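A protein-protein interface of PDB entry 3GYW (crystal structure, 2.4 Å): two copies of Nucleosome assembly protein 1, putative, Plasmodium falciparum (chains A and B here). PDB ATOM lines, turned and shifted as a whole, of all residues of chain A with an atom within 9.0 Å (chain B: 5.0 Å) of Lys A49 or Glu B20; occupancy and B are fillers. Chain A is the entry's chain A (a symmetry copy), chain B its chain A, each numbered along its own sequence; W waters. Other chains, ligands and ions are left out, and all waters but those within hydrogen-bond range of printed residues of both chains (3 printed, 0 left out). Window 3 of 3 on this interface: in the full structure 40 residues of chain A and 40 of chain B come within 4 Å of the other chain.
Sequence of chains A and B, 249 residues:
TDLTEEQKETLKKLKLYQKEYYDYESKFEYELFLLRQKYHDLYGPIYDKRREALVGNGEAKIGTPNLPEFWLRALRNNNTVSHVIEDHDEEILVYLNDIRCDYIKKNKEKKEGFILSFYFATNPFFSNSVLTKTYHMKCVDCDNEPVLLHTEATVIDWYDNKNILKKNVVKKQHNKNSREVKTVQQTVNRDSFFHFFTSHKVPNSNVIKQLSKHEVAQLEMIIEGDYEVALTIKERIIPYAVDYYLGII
O of Tyr A47 lies within hydrogen-bond range of NH2 of Arg A100.
Water W3 lies within hydrogen-bond range of the backbone carbonyl oxygen (O) of Pro A239, the guanidinium group (NH2) of Arg A50 and the side-chain amide nitrogen (NE2) of Gln B18. Water W2 lies within hydrogen-bond range of the side-chain amide nitrogen of Gln B18 and the guanidinium group of Arg A50. Water W1 lies within hydrogen-bond range of O of Lys A49 (2.7 Å), OH of Tyr B17 (2.9 Å) and N of Ala A53 (3.4 Å).
Of chain B, only Tyr B17 and Glu B20 come within 4 Å of Lys A49. Of the printed residues of chain B, Arg A50 touches Tyr B17. Printed residues of chain A within 4 Å of Tyr B24: Tyr A39, Leu A42, Tyr A43 and Ile A46. Of the printed residues of chain B, Ile A46 touches Tyr B17, Glu B20, Tyr B21 and Tyr B24. Of the printed residues of chain B, Pro A239 touches Gln B18 and Tyr B21. Of the printed residues of chain A, Gln B18 touches Pro A239 (2.9 Å). Asp A48 touches none of the printed residues of chain B. The nearest printed residue of chain B that does not touch Lys A49 is Leu B16 (6.1 Å). The nearest residue of chain A that does not touch Glu B20 is Leu A42 (5.9 Å). The nearest printed residue of chain B that does not touch Tyr A47 is Tyr B17 (6.4 Å).
Among the printed residues, pairs that only touch across the chains: Tyr A39 with Tyr B24, Leu A42 with Tyr B24, Tyr A43 with Tyr B21, Tyr A43 with Tyr B24, Ile A46 with Tyr B17, Ile A46 with Glu B20, Ile A46 with Tyr B21, Ile A46 with Tyr B24, Tyr A47 with Tyr B21, Lys A49 with Tyr B17, Arg A50 with Tyr B17 and Pro A239 with Tyr B21.
OE1 of Gln B18 sits close to O of Pro A239. The side-chain amino group (NZ) of Lys A49 is in salt-bridge range of the side-chain carboxylate (OE1) of Glu B20 (2.8 Å).
Hydrophobic or aromatic side chains of chain A that line the printed part of chain B: Tyr A39, Leu A42, Tyr A43, Ile A46, Tyr A47 and Pro A239. Along chain A the printed residues that touch a printed residue of chain B span positions 39 to 239. Hydrophobic or aromatic side chains of chain B that line the printed part of chain A: Tyr B17, Tyr B21 and Tyr B24. Among the printed residues, 14 pairs touch across the chains. Among the printed residues, Asp or Glu carboxylates within 4 Å of a Lys or Arg side-chain nitrogen of the other chain: Lys A49 with Glu B20.
No position is printed for both chains. Of the 14 pairs that touch across the chains among the printed residues, none has its exchanged pair printed and touching as well.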
ATOM      1  N   TYR A  39      -3.630  -5.537  -9.495  1.00  0.00           N
ATOM      2  CA  TYR A  39      -3.864  -6.563 -10.502  1.00  0.00           C
ATOM      3  C   TYR A  39      -4.924  -7.612 -10.137  1.00  0.00           C
ATOM      4  O   TYR A  39      -5.552  -8.181 -11.026  1.00  0.00           O
ATOM      5  CB  TYR A  39      -2.540  -7.170 -10.985  1.00  0.00           C
ATOM      6  CG  TYR A  39      -1.876  -6.252 -11.983  1.00  0.00           C
ATOM      7  CD1 TYR A  39      -2.204  -6.317 -13.340  1.00  0.00           C
ATOM      8  CD2 TYR A  39      -0.967  -5.278 -11.568  1.00  0.00           C
ATOM      9  CE1 TYR A  39      -1.624  -5.457 -14.255  1.00  0.00           C
ATOM     10  CE2 TYR A  39      -0.379  -4.414 -12.479  1.00  0.00           C
ATOM     11  CZ  TYR A  39      -0.713  -4.508 -13.820  1.00  0.00           C
ATOM     12  OH  TYR A  39      -0.143  -3.653 -14.730  1.00  0.00           O
ATOM     13  N   LEU A  42      -7.907  -5.876 -11.304  1.00  0.00           N
ATOM     14  CA  LEU A  42      -7.939  -5.952 -12.767  1.00  0.00           C
ATOM     15  C   LEU A  42      -8.320  -7.355 -13.278  1.00  0.00           C
ATOM     16  O   LEU A  42      -8.899  -7.475 -14.358  1.00  0.00           O
ATOM     17  CB  LEU A  42      -6.620  -5.474 -13.393  1.00  0.00           C
ATOM     18  CG  LEU A  42      -6.346  -3.959 -13.434  1.00  0.00           C
ATOM     19  CD1 LEU A  42      -4.897  -3.674 -13.845  1.00  0.00           C
ATOM     20  CD2 LEU A  42      -7.333  -3.211 -14.347  1.00  0.00           C
ATOM     21  N   TYR A  43      -8.011  -8.401 -12.509  1.00  0.00           N
ATOM     22  CA  TYR A  43      -8.423  -9.764 -12.877  1.00  0.00           C
ATOM     23  C   TYR A  43      -9.897 -10.031 -12.590  1.00  0.00           C
ATOM     24  O   TYR A  43     -10.528 -10.825 -13.291  1.00  0.00           O
ATOM     25  CB  TYR A  43      -7.574 -10.840 -12.189  1.00  0.00           C
ATOM     26  CG  TYR A  43      -6.082 -10.760 -12.436  1.00  0.00           C
ATOM     27  CD1 TYR A  43      -5.568 -10.436 -13.696  1.00  0.00           C
ATOM     28  CD2 TYR A  43      -5.181 -11.027 -11.403  1.00  0.00           C
ATOM     29  CE1 TYR A  43      -4.188 -10.367 -13.917  1.00  0.00           C
ATOM     30  CE2 TYR A  43      -3.805 -10.965 -11.609  1.00  0.00           C
ATOM     31  CZ  TYR A  43      -3.312 -10.635 -12.866  1.00  0.00           C
ATOM     32  OH  TYR A  43      -1.948 -10.576 -13.058  1.00  0.00           O
ATOM     33  N   GLY A  44     -10.428  -9.378 -11.555  1.00  0.00           N
ATOM     34  CA  GLY A  44     -11.831  -9.507 -11.144  1.00  0.00           C
ATOM     35  C   GLY A  44     -12.889  -9.544 -12.242  1.00  0.00           C
ATOM     36  O   GLY A  44     -13.666 -10.497 -12.300  1.00  0.00           O
ATOM     37  N   PRO A  45     -12.944  -8.506 -13.111  1.00  0.00           N
ATOM     38  CA  PRO A  45     -13.932  -8.479 -14.199  1.00  0.00           C
ATOM     39  C   PRO A  45     -13.786  -9.627 -15.204  1.00  0.00           C
ATOM     40  O   PRO A  45     -14.787 -10.107 -15.724  1.00  0.00           O
ATOM     41  CB  PRO A  45     -13.663  -7.133 -14.895  1.00  0.00           C
ATOM     42  CG  PRO A  45     -12.954  -6.308 -13.879  1.00  0.00           C
ATOM     43  CD  PRO A  45     -12.112  -7.289 -13.125  1.00  0.00           C
ATOM     44  N   ILE A  46     -12.552 -10.048 -15.471  1.00  0.00           N
ATOM     45  CA  ILE A  46     -12.279 -11.164 -16.380  1.00  0.00           C
ATOM     46  C   ILE A  46     -12.867 -12.469 -15.833  1.00  0.00           C
ATOM     47  O   ILE A  46     -13.470 -13.254 -16.582  1.00  0.00           O
ATOM     48  CB  ILE A  46     -10.760 -11.315 -16.661  1.00  0.00           C
ATOM     49  CG1 ILE A  46     -10.210 -10.043 -17.318  1.00  0.00           C
ATOM     50  CG2 ILE A  46     -10.482 -12.549 -17.533  1.00  0.00           C
ATOM     51  CD1 ILE A  46      -8.686  -9.955 -17.372  1.00  0.00           C
ATOM     52  N   TYR A  47     -12.699 -12.689 -14.528  1.00  0.00           N
ATOM     53  CA  TYR A  47     -13.319 -13.823 -13.855  1.00  0.00           C
ATOM     54  C   TYR A  47     -14.838 -13.739 -13.910  1.00  0.00           C
ATOM     55  O   TYR A  47     -15.508 -14.749 -14.124  1.00  0.00           O
ATOM     56  CB  TYR A  47     -12.862 -13.930 -12.395  1.00  0.00           C
ATOM     57  CG  TYR A  47     -11.372 -14.091 -12.202  1.00  0.00           C
ATOM     58  CD1 TYR A  47     -10.604 -14.831 -13.101  1.00  0.00           C
ATOM     59  CD2 TYR A  47     -10.734 -13.511 -11.107  1.00  0.00           C
ATOM     60  CE1 TYR A  47      -9.239 -14.976 -12.925  1.00  0.00           C
ATOM     61  CE2 TYR A  47      -9.375 -13.661 -10.914  1.00  0.00           C
ATOM     62  CZ  TYR A  47      -8.631 -14.391 -11.827  1.00  0.00           C
ATOM     63  OH  TYR A  47      -7.270 -14.537 -11.640  1.00  0.00           O
ATOM     64  N   ASP A  48     -15.370 -12.536 -13.701  1.00  0.00           N
ATOM     65  CA  ASP A  48     -16.808 -12.282 -13.772  1.00  0.00           C
ATOM     66  C   ASP A  48     -17.367 -12.592 -15.149  1.00  0.00           C
ATOM     67  O   ASP A  48     -18.412 -13.234 -15.268  1.00  0.00           O
ATOM     68  CB  ASP A  48     -17.121 -10.827 -13.407  1.00  0.00           C
ATOM     69  CG  ASP A  48     -16.958 -10.546 -11.931  1.00  0.00           C
ATOM     70  OD1 ASP A  48     -16.866 -11.516 -11.156  1.00  0.00           O
ATOM     71  OD2 ASP A  48     -16.921  -9.358 -11.539  1.00  0.00           O
ATOM     72  N   LYS A  49     -16.665 -12.136 -16.184  1.00  0.00           N
ATOM     73  CA  LYS A  49     -17.097 -12.352 -17.565  1.00  0.00           C
ATOM     74  C   LYS A  49     -17.117 -13.835 -17.902  1.00  0.00           C
ATOM     75  O   LYS A  49     -18.073 -14.328 -18.506  1.00  0.00           O
ATOM     76  CB  LYS A  49     -16.206 -11.586 -18.549  1.00  0.00           C
ATOM     77  CG  LYS A  49     -16.462 -10.088 -18.588  1.00  0.00           C
ATOM     78  CD  LYS A  49     -15.748  -9.398 -19.770  1.00  0.00           C
ATOM     79  CE  LYS A  49     -14.226  -9.382 -19.608  1.00  0.00           C
ATOM     80  NZ  LYS A  49     -13.544  -8.479 -20.583  1.00  0.00           N
ATOM     81  N   ARG A  50     -16.062 -14.535 -17.493  1.00  0.00           N
ATOM     82  CA  ARG A  50     -15.949 -15.976 -17.695  1.00  0.00           C
ATOM     83  C   ARG A  50     -17.129 -16.701 -17.055  1.00  0.00           C
ATOM     84  O   ARG A  50     -17.800 -17.486 -17.717  1.00  0.00           O
ATOM     85  CB  ARG A  50     -14.627 -16.487 -17.129  1.00  0.00           C
ATOM     86  CG  ARG A  50     -14.496 -18.000 -17.079  1.00  0.00           C
ATOM     87  CD  ARG A  50     -13.712 -18.414 -15.851  1.00  0.00           C
ATOM     88  NE  ARG A  50     -12.280 -18.432 -16.094  1.00  0.00           N
ATOM     89  CZ  ARG A  50     -11.347 -18.291 -15.157  1.00  0.00           C
ATOM     90  NH1 ARG A  50     -11.674 -18.103 -13.883  1.00  0.00           N
ATOM     91  NH2 ARG A  50     -10.072 -18.339 -15.509  1.00  0.00           N
ATOM     92  N   ARG A  51     -17.378 -16.414 -15.775  1.00  0.00           N
ATOM     93  CA  ARG A  51     -18.509 -16.989 -15.050  1.00  0.00           C
ATOM     94  C   ARG A  51     -19.847 -16.709 -15.748  1.00  0.00           C
ATOM     95  O   ARG A  51     -20.661 -17.618 -15.917  1.00  0.00           O
ATOM     96  CB  ARG A  51     -18.549 -16.483 -13.605  1.00  0.00           C
ATOM     97  CG  ARG A  51     -19.593 -17.188 -12.742  1.00  0.00           C
ATOM     98  CD  ARG A  51     -20.103 -16.304 -11.617  1.00  0.00           C
ATOM     99  NE  ARG A  51     -20.859 -15.161 -12.120  1.00  0.00           N
ATOM    100  CZ  ARG A  51     -20.586 -13.883 -11.850  1.00  0.00           C
ATOM    101  NH1 ARG A  51     -19.570 -13.554 -11.051  1.00  0.00           N
ATOM    102  NH2 ARG A  51     -21.348 -12.924 -12.373  1.00  0.00           N
ATOM    103  N   GLU A  52     -20.057 -15.454 -16.145  1.00  0.00           N
ATOM    104  CA  GLU A  52     -21.250 -15.039 -16.878  1.00  0.00           C
ATOM    105  C   GLU A  52     -21.448 -15.850 -18.172  1.00  0.00           C
ATOM    106  O   GLU A  52     -22.557 -16.305 -18.462  1.00  0.00           O
ATOM    107  CB  GLU A  52     -21.186 -13.531 -17.155  1.00  0.00           C
ATOM    108  CG  GLU A  52     -22.259 -12.966 -18.088  1.00  0.00           C
ATOM    109  CD  GLU A  52     -23.681 -13.156 -17.567  1.00  0.00           C
ATOM    110  OE1 GLU A  52     -23.914 -12.992 -16.343  1.00  0.00           O
ATOM    111  OE2 GLU A  52     -24.568 -13.465 -18.393  1.00  0.00           O
ATOM    112  N   ALA A  53     -20.372 -16.056 -18.925  1.00  0.00           N
ATOM    113  CA  ALA A  53     -20.445 -16.823 -20.162  1.00  0.00           C
ATOM    114  C   ALA A  53     -20.731 -18.305 -19.910  1.00  0.00           C
ATOM    115  O   ALA A  53     -21.465 -18.936 -20.667  1.00  0.00           O
ATOM    116  CB  ALA A  53     -19.173 -16.647 -20.979  1.00  0.00           C
ATOM    117  N   LEU A  54     -20.160 -18.844 -18.835  1.00  0.00           N
ATOM    118  CA  LEU A  54     -20.293 -20.259 -18.490  1.00  0.00           C
ATOM    119  C   LEU A  54     -21.675 -20.610 -17.946  1.00  0.00           C
ATOM    120  O   LEU A  54     -22.253 -21.640 -18.299  1.00  0.00           O
ATOM    121  CB  LEU A  54     -19.234 -20.652 -17.453  1.00  0.00           C
ATOM    122  CG  LEU A  54     -17.790 -20.868 -17.899  1.00  0.00           C
ATOM    123  CD1 LEU A  54     -16.907 -21.040 -16.686  1.00  0.00           C
ATOM    124  CD2 LEU A  54     -17.660 -22.055 -18.833  1.00  0.00           C
ATOM    125  N   VAL A  55     -22.191 -19.735 -17.090  1.00  0.00           N
ATOM    126  CA  VAL A  55     -23.383 -20.013 -16.303  1.00  0.00           C
ATOM    127  C   VAL A  55     -24.628 -19.372 -16.917  1.00  0.00           C
ATOM    128  O   VAL A  55     -25.646 -20.037 -17.090  1.00  0.00           O
ATOM    129  CB  VAL A  55     -23.190 -19.552 -14.826  1.00  0.00           C
ATOM    130  CG1 VAL A  55     -24.467 -19.723 -14.020  1.00  0.00           C
ATOM    131  CG2 VAL A  55     -22.045 -20.320 -14.179  1.00  0.00           C
ATOM    132  N   GLY A  56     -24.531 -18.089 -17.255  1.00  0.00           N
ATOM    133  CA  GLY A  56     -25.678 -17.313 -17.711  1.00  0.00           C
ATOM    134  C   GLY A  56     -26.106 -16.338 -16.630  1.00  0.00           C
ATOM    135  O   GLY A  56     -27.036 -16.608 -15.861  1.00  0.00           O
ATOM    136  N   ASN A  66     -23.667 -23.468 -20.037  1.00  0.00           N
ATOM    137  CA  ASN A  66     -23.229 -23.014 -21.361  1.00  0.00           C
ATOM    138  C   ASN A  66     -22.004 -23.754 -21.891  1.00  0.00           C
ATOM    139  O   ASN A  66     -21.698 -23.678 -23.083  1.00  0.00           O
ATOM    140  CB  ASN A  66     -22.981 -21.505 -21.374  1.00  0.00           C
ATOM    141  CG  ASN A  66     -24.256 -20.697 -21.189  1.00  0.00           C
ATOM    142  OD1 ASN A  66     -25.353 -21.148 -21.534  1.00  0.00           O
ATOM    143  ND2 ASN A  66     -24.115 -19.493 -20.648  1.00  0.00           N
ATOM    144  N   ASP A  98     -18.526 -22.054 -10.537  1.00  0.00           N
ATOM    145  CA  ASP A  98     -17.402 -21.116 -10.447  1.00  0.00           C
ATOM    146  C   ASP A  98     -16.463 -21.445  -9.293  1.00  0.00           C
ATOM    147  O   ASP A  98     -16.891 -21.944  -8.242  1.00  0.00           O
ATOM    148  CB  ASP A  98     -17.923 -19.684 -10.287  1.00  0.00           C
ATOM    149  CG  ASP A  98     -16.924 -18.625 -10.745  1.00  0.00           C
ATOM    150  OD1 ASP A  98     -15.908 -18.967 -11.394  1.00  0.00           O
ATOM    151  OD2 ASP A  98     -17.163 -17.432 -10.451  1.00  0.00           O
ATOM    152  N   ARG A 100     -13.620 -19.244  -7.095  1.00  0.00           N
ATOM    153  CA  ARG A 100     -13.089 -17.898  -6.823  1.00  0.00           C
ATOM    154  C   ARG A 100     -12.018 -17.874  -5.729  1.00  0.00           C
ATOM    155  O   ARG A 100     -11.915 -18.793  -4.912  1.00  0.00           O
ATOM    156  CB  ARG A 100     -14.220 -16.937  -6.426  1.00  0.00           C
ATOM    157  CG  ARG A 100     -15.206 -16.612  -7.531  1.00  0.00           C
ATOM    158  CD  ARG A 100     -14.722 -15.447  -8.375  1.00  0.00           C
ATOM    159  NE  ARG A 100     -15.521 -15.323  -9.589  1.00  0.00           N
ATOM    160  CZ  ARG A 100     -15.704 -14.193 -10.264  1.00  0.00           C
ATOM    161  NH1 ARG A 100     -15.140 -13.057  -9.858  1.00  0.00           N
ATOM    162  NH2 ARG A 100     -16.464 -14.206 -11.346  1.00  0.00           N
ATOM    163  N   PRO A 239      -6.435 -18.640 -12.539  1.00  0.00           N
ATOM    164  CA  PRO A 239      -5.868 -17.787 -13.593  1.00  0.00           C
ATOM    165  C   PRO A 239      -5.914 -18.365 -15.013  1.00  0.00           C
ATOM    166  O   PRO A 239      -6.085 -17.605 -15.968  1.00  0.00           O
ATOM    167  CB  PRO A 239      -4.408 -17.606 -13.148  1.00  0.00           C
ATOM    168  CG  PRO A 239      -4.426 -17.887 -11.676  1.00  0.00           C
ATOM    169  CD  PRO A 239      -5.402 -19.015 -11.558  1.00  0.00           C
ATOM    170  N   LEU B  16     -10.999 -15.486 -25.549  1.00  0.00           N
ATOM    171  CA  LEU B  16     -10.833 -14.033 -25.560  1.00  0.00           C
ATOM    172  C   LEU B  16     -10.472 -13.497 -24.169  1.00  0.00           C
ATOM    173  O   LEU B  16      -9.525 -12.731 -24.034  1.00  0.00           O
ATOM    174  CB  LEU B  16     -12.094 -13.331 -26.102  1.00  0.00           C
ATOM    175  CG  LEU B  16     -12.158 -11.791 -26.032  1.00  0.00           C
ATOM    176  CD1 LEU B  16     -11.398 -11.132 -27.187  1.00  0.00           C
ATOM    177  CD2 LEU B  16     -13.599 -11.281 -25.988  1.00  0.00           C
ATOM    178  N   TYR B  17     -11.227 -13.909 -23.150  1.00  0.00           N
ATOM    179  CA  TYR B  17     -10.981 -13.455 -21.783  1.00  0.00           C
ATOM    180  C   TYR B  17      -9.644 -13.947 -21.227  1.00  0.00           C
ATOM    181  O   TYR B  17      -9.008 -13.245 -20.452  1.00  0.00           O
ATOM    182  CB  TYR B  17     -12.109 -13.875 -20.829  1.00  0.00           C
ATOM    183  CG  TYR B  17     -13.522 -13.563 -21.281  1.00  0.00           C
ATOM    184  CD1 TYR B  17     -13.819 -12.398 -21.996  1.00  0.00           C
ATOM    185  CD2 TYR B  17     -14.572 -14.420 -20.953  1.00  0.00           C
ATOM    186  CE1 TYR B  17     -15.118 -12.113 -22.395  1.00  0.00           C
ATOM    187  CE2 TYR B  17     -15.875 -14.142 -21.344  1.00  0.00           C
ATOM    188  CZ  TYR B  17     -16.139 -12.987 -22.067  1.00  0.00           C
ATOM    189  OH  TYR B  17     -17.431 -12.709 -22.453  1.00  0.00           O
ATOM    190  N   GLN B  18      -9.232 -15.149 -21.618  1.00  0.00           N
ATOM    191  CA  GLN B  18      -7.960 -15.712 -21.167  1.00  0.00           C
ATOM    192  C   GLN B  18      -6.768 -14.959 -21.758  1.00  0.00           C
ATOM    193  O   GLN B  18      -5.771 -14.724 -21.068  1.00  0.00           O
ATOM    194  CB  GLN B  18      -7.867 -17.210 -21.493  1.00  0.00           C
ATOM    195  CG  GLN B  18      -6.657 -17.914 -20.891  1.00  0.00           C
ATOM    196  CD  GLN B  18      -6.600 -17.804 -19.368  1.00  0.00           C
ATOM    197  OE1 GLN B  18      -5.711 -17.155 -18.816  1.00  0.00           O
ATOM    198  NE2 GLN B  18      -7.556 -18.428 -18.688  1.00  0.00           N
ATOM    199  N   LYS B  19      -6.879 -14.589 -23.033  1.00  0.00           N
ATOM    200  CA  LYS B  19      -5.877 -13.748 -23.674  1.00  0.00           C
ATOM    201  C   LYS B  19      -5.813 -12.382 -22.980  1.00  0.00           C
ATOM    202  O   LYS B  19      -4.726 -11.826 -22.783  1.00  0.00           O
ATOM    203  CB  LYS B  19      -6.151 -13.602 -25.175  1.00  0.00           C
ATOM    204  CG  LYS B  19      -5.208 -12.640 -25.898  1.00  0.00           C
ATOM    205  CD  LYS B  19      -3.754 -13.118 -25.863  1.00  0.00           C
ATOM    206  CE  LYS B  19      -2.798 -12.017 -26.348  1.00  0.00           C
ATOM    207  NZ  LYS B  19      -1.500 -12.564 -26.873  1.00  0.00           N
ATOM    208  N   GLU B  20      -6.971 -11.857 -22.590  1.00  0.00           N
ATOM    209  CA  GLU B  20      -7.006 -10.628 -21.816  1.00  0.00           C
ATOM    210  C   GLU B  20      -6.306 -10.781 -20.459  1.00  0.00           C
ATOM    211  O   GLU B  20      -5.570  -9.885 -20.036  1.00  0.00           O
ATOM    212  CB  GLU B  20      -8.432 -10.105 -21.643  1.00  0.00           C
ATOM    213  CG  GLU B  20      -8.458  -8.629 -21.305  1.00  0.00           C
ATOM    214  CD  GLU B  20      -9.776  -8.146 -20.753  1.00  0.00           C
ATOM    215  OE1 GLU B  20     -10.790  -8.854 -20.887  1.00  0.00           O
ATOM    216  OE2 GLU B  20      -9.799  -7.036 -20.187  1.00  0.00           O
ATOM    217  N   TYR B  21      -6.520 -11.916 -19.794  1.00  0.00           N
ATOM    218  CA  TYR B  21      -5.821 -12.208 -18.540  1.00  0.00           C
ATOM    219  C   TYR B  21      -4.307 -12.163 -18.723  1.00  0.00           C
ATOM    220  O   TYR B  21      -3.601 -11.579 -17.895  1.00  0.00           O
ATOM    221  CB  TYR B  21      -6.228 -13.558 -17.935  1.00  0.00           C
ATOM    222  CG  TYR B  21      -5.472 -13.853 -16.656  1.00  0.00           C
ATOM    223  CD1 TYR B  21      -6.007 -13.510 -15.414  1.00  0.00           C
ATOM    224  CD2 TYR B  21      -4.202 -14.438 -16.688  1.00  0.00           C
ATOM    225  CE1 TYR B  21      -5.302 -13.758 -14.233  1.00  0.00           C
ATOM    226  CE2 TYR B  21      -3.490 -14.682 -15.516  1.00  0.00           C
ATOM    227  CZ  TYR B  21      -4.045 -14.342 -14.297  1.00  0.00           C
ATOM    228  OH  TYR B  21      -3.343 -14.588 -13.135  1.00  0.00           O
ATOM    229  N   TYR B  22      -3.827 -12.787 -19.803  1.00  0.00           N
ATOM    230  CA  TYR B  22      -2.397 -12.839 -20.133  1.00  0.00           C
ATOM    231  C   TYR B  22      -1.814 -11.480 -20.461  1.00  0.00           C
ATOM    232  O   TYR B  22      -0.655 -11.223 -20.160  1.00  0.00           O
ATOM    233  CB  TYR B  22      -2.131 -13.794 -21.298  1.00  0.00           C
ATOM    234  CG  TYR B  22      -2.265 -15.252 -20.944  1.00  0.00           C
ATOM    235  CD1 TYR B  22      -1.670 -15.771 -19.792  1.00  0.00           C
ATOM    236  CD2 TYR B  22      -2.968 -16.122 -21.770  1.00  0.00           C
ATOM    237  CE1 TYR B  22      -1.791 -17.124 -19.465  1.00  0.00           C
ATOM    238  CE2 TYR B  22      -3.091 -17.474 -21.456  1.00  0.00           C
ATOM    239  CZ  TYR B  22      -2.504 -17.962 -20.301  1.00  0.00           C
ATOM    240  OH  TYR B  22      -2.626 -19.294 -19.992  1.00  0.00           O
ATOM    241  N   ASP B  23      -2.618 -10.620 -21.083  1.00  0.00           N
ATOM    242  CA  ASP B  23      -2.240  -9.234 -21.328  1.00  0.00           C
ATOM    243  C   ASP B  23      -1.906  -8.530 -20.010  1.00  0.00           C
ATOM    244  O   ASP B  23      -0.842  -7.921 -19.882  1.00  0.00           O
ATOM    245  CB  ASP B  23      -3.364  -8.481 -22.047  1.00  0.00           C
ATOM    246  CG  ASP B  23      -3.477  -8.842 -23.525  1.00  0.00           C
ATOM    247  OD1 ASP B  23      -2.549  -9.475 -24.082  1.00  0.00           O
ATOM    248  OD2 ASP B  23      -4.511  -8.468 -24.133  1.00  0.00           O
ATOM    249  N   TYR B  24      -2.819  -8.634 -19.043  1.00  0.00           N
ATOM    250  CA  TYR B  24      -2.659  -8.034 -17.722  1.00  0.00           C
ATOM    251  C   TYR B  24      -1.542  -8.674 -16.901  1.00  0.00           C
ATOM    252  O   TYR B  24      -0.782  -7.968 -16.243  1.00  0.00           O
ATOM    253  CB  TYR B  24      -3.967  -8.102 -16.933  1.00  0.00           C
ATOM    254  CG  TYR B  24      -5.000  -7.070 -17.324  1.00  0.00           C
ATOM    255  CD1 TYR B  24      -4.711  -5.703 -17.278  1.00  0.00           C
ATOM    256  CD2 TYR B  24      -6.276  -7.457 -17.712  1.00  0.00           C
ATOM    257  CE1 TYR B  24      -5.669  -4.746 -17.634  1.00  0.00           C
ATOM    258  CE2 TYR B  24      -7.239  -6.519 -18.067  1.00  0.00           C
ATOM    259  CZ  TYR B  24      -6.932  -5.166 -18.025  1.00  0.00           C
ATOM    260  OH  TYR B  24      -7.897  -4.247 -18.368  1.00  0.00           O
HETATM  261  O   HOH W   1     -19.543 -13.125 -20.463  1.00  0.00           O
HETATM  262  O   HOH W   2      -9.985 -19.302 -18.076  1.00  0.00           O
HETATM  263  O   HOH W   3      -8.125 -16.052 -16.254  1.00  0.00           O
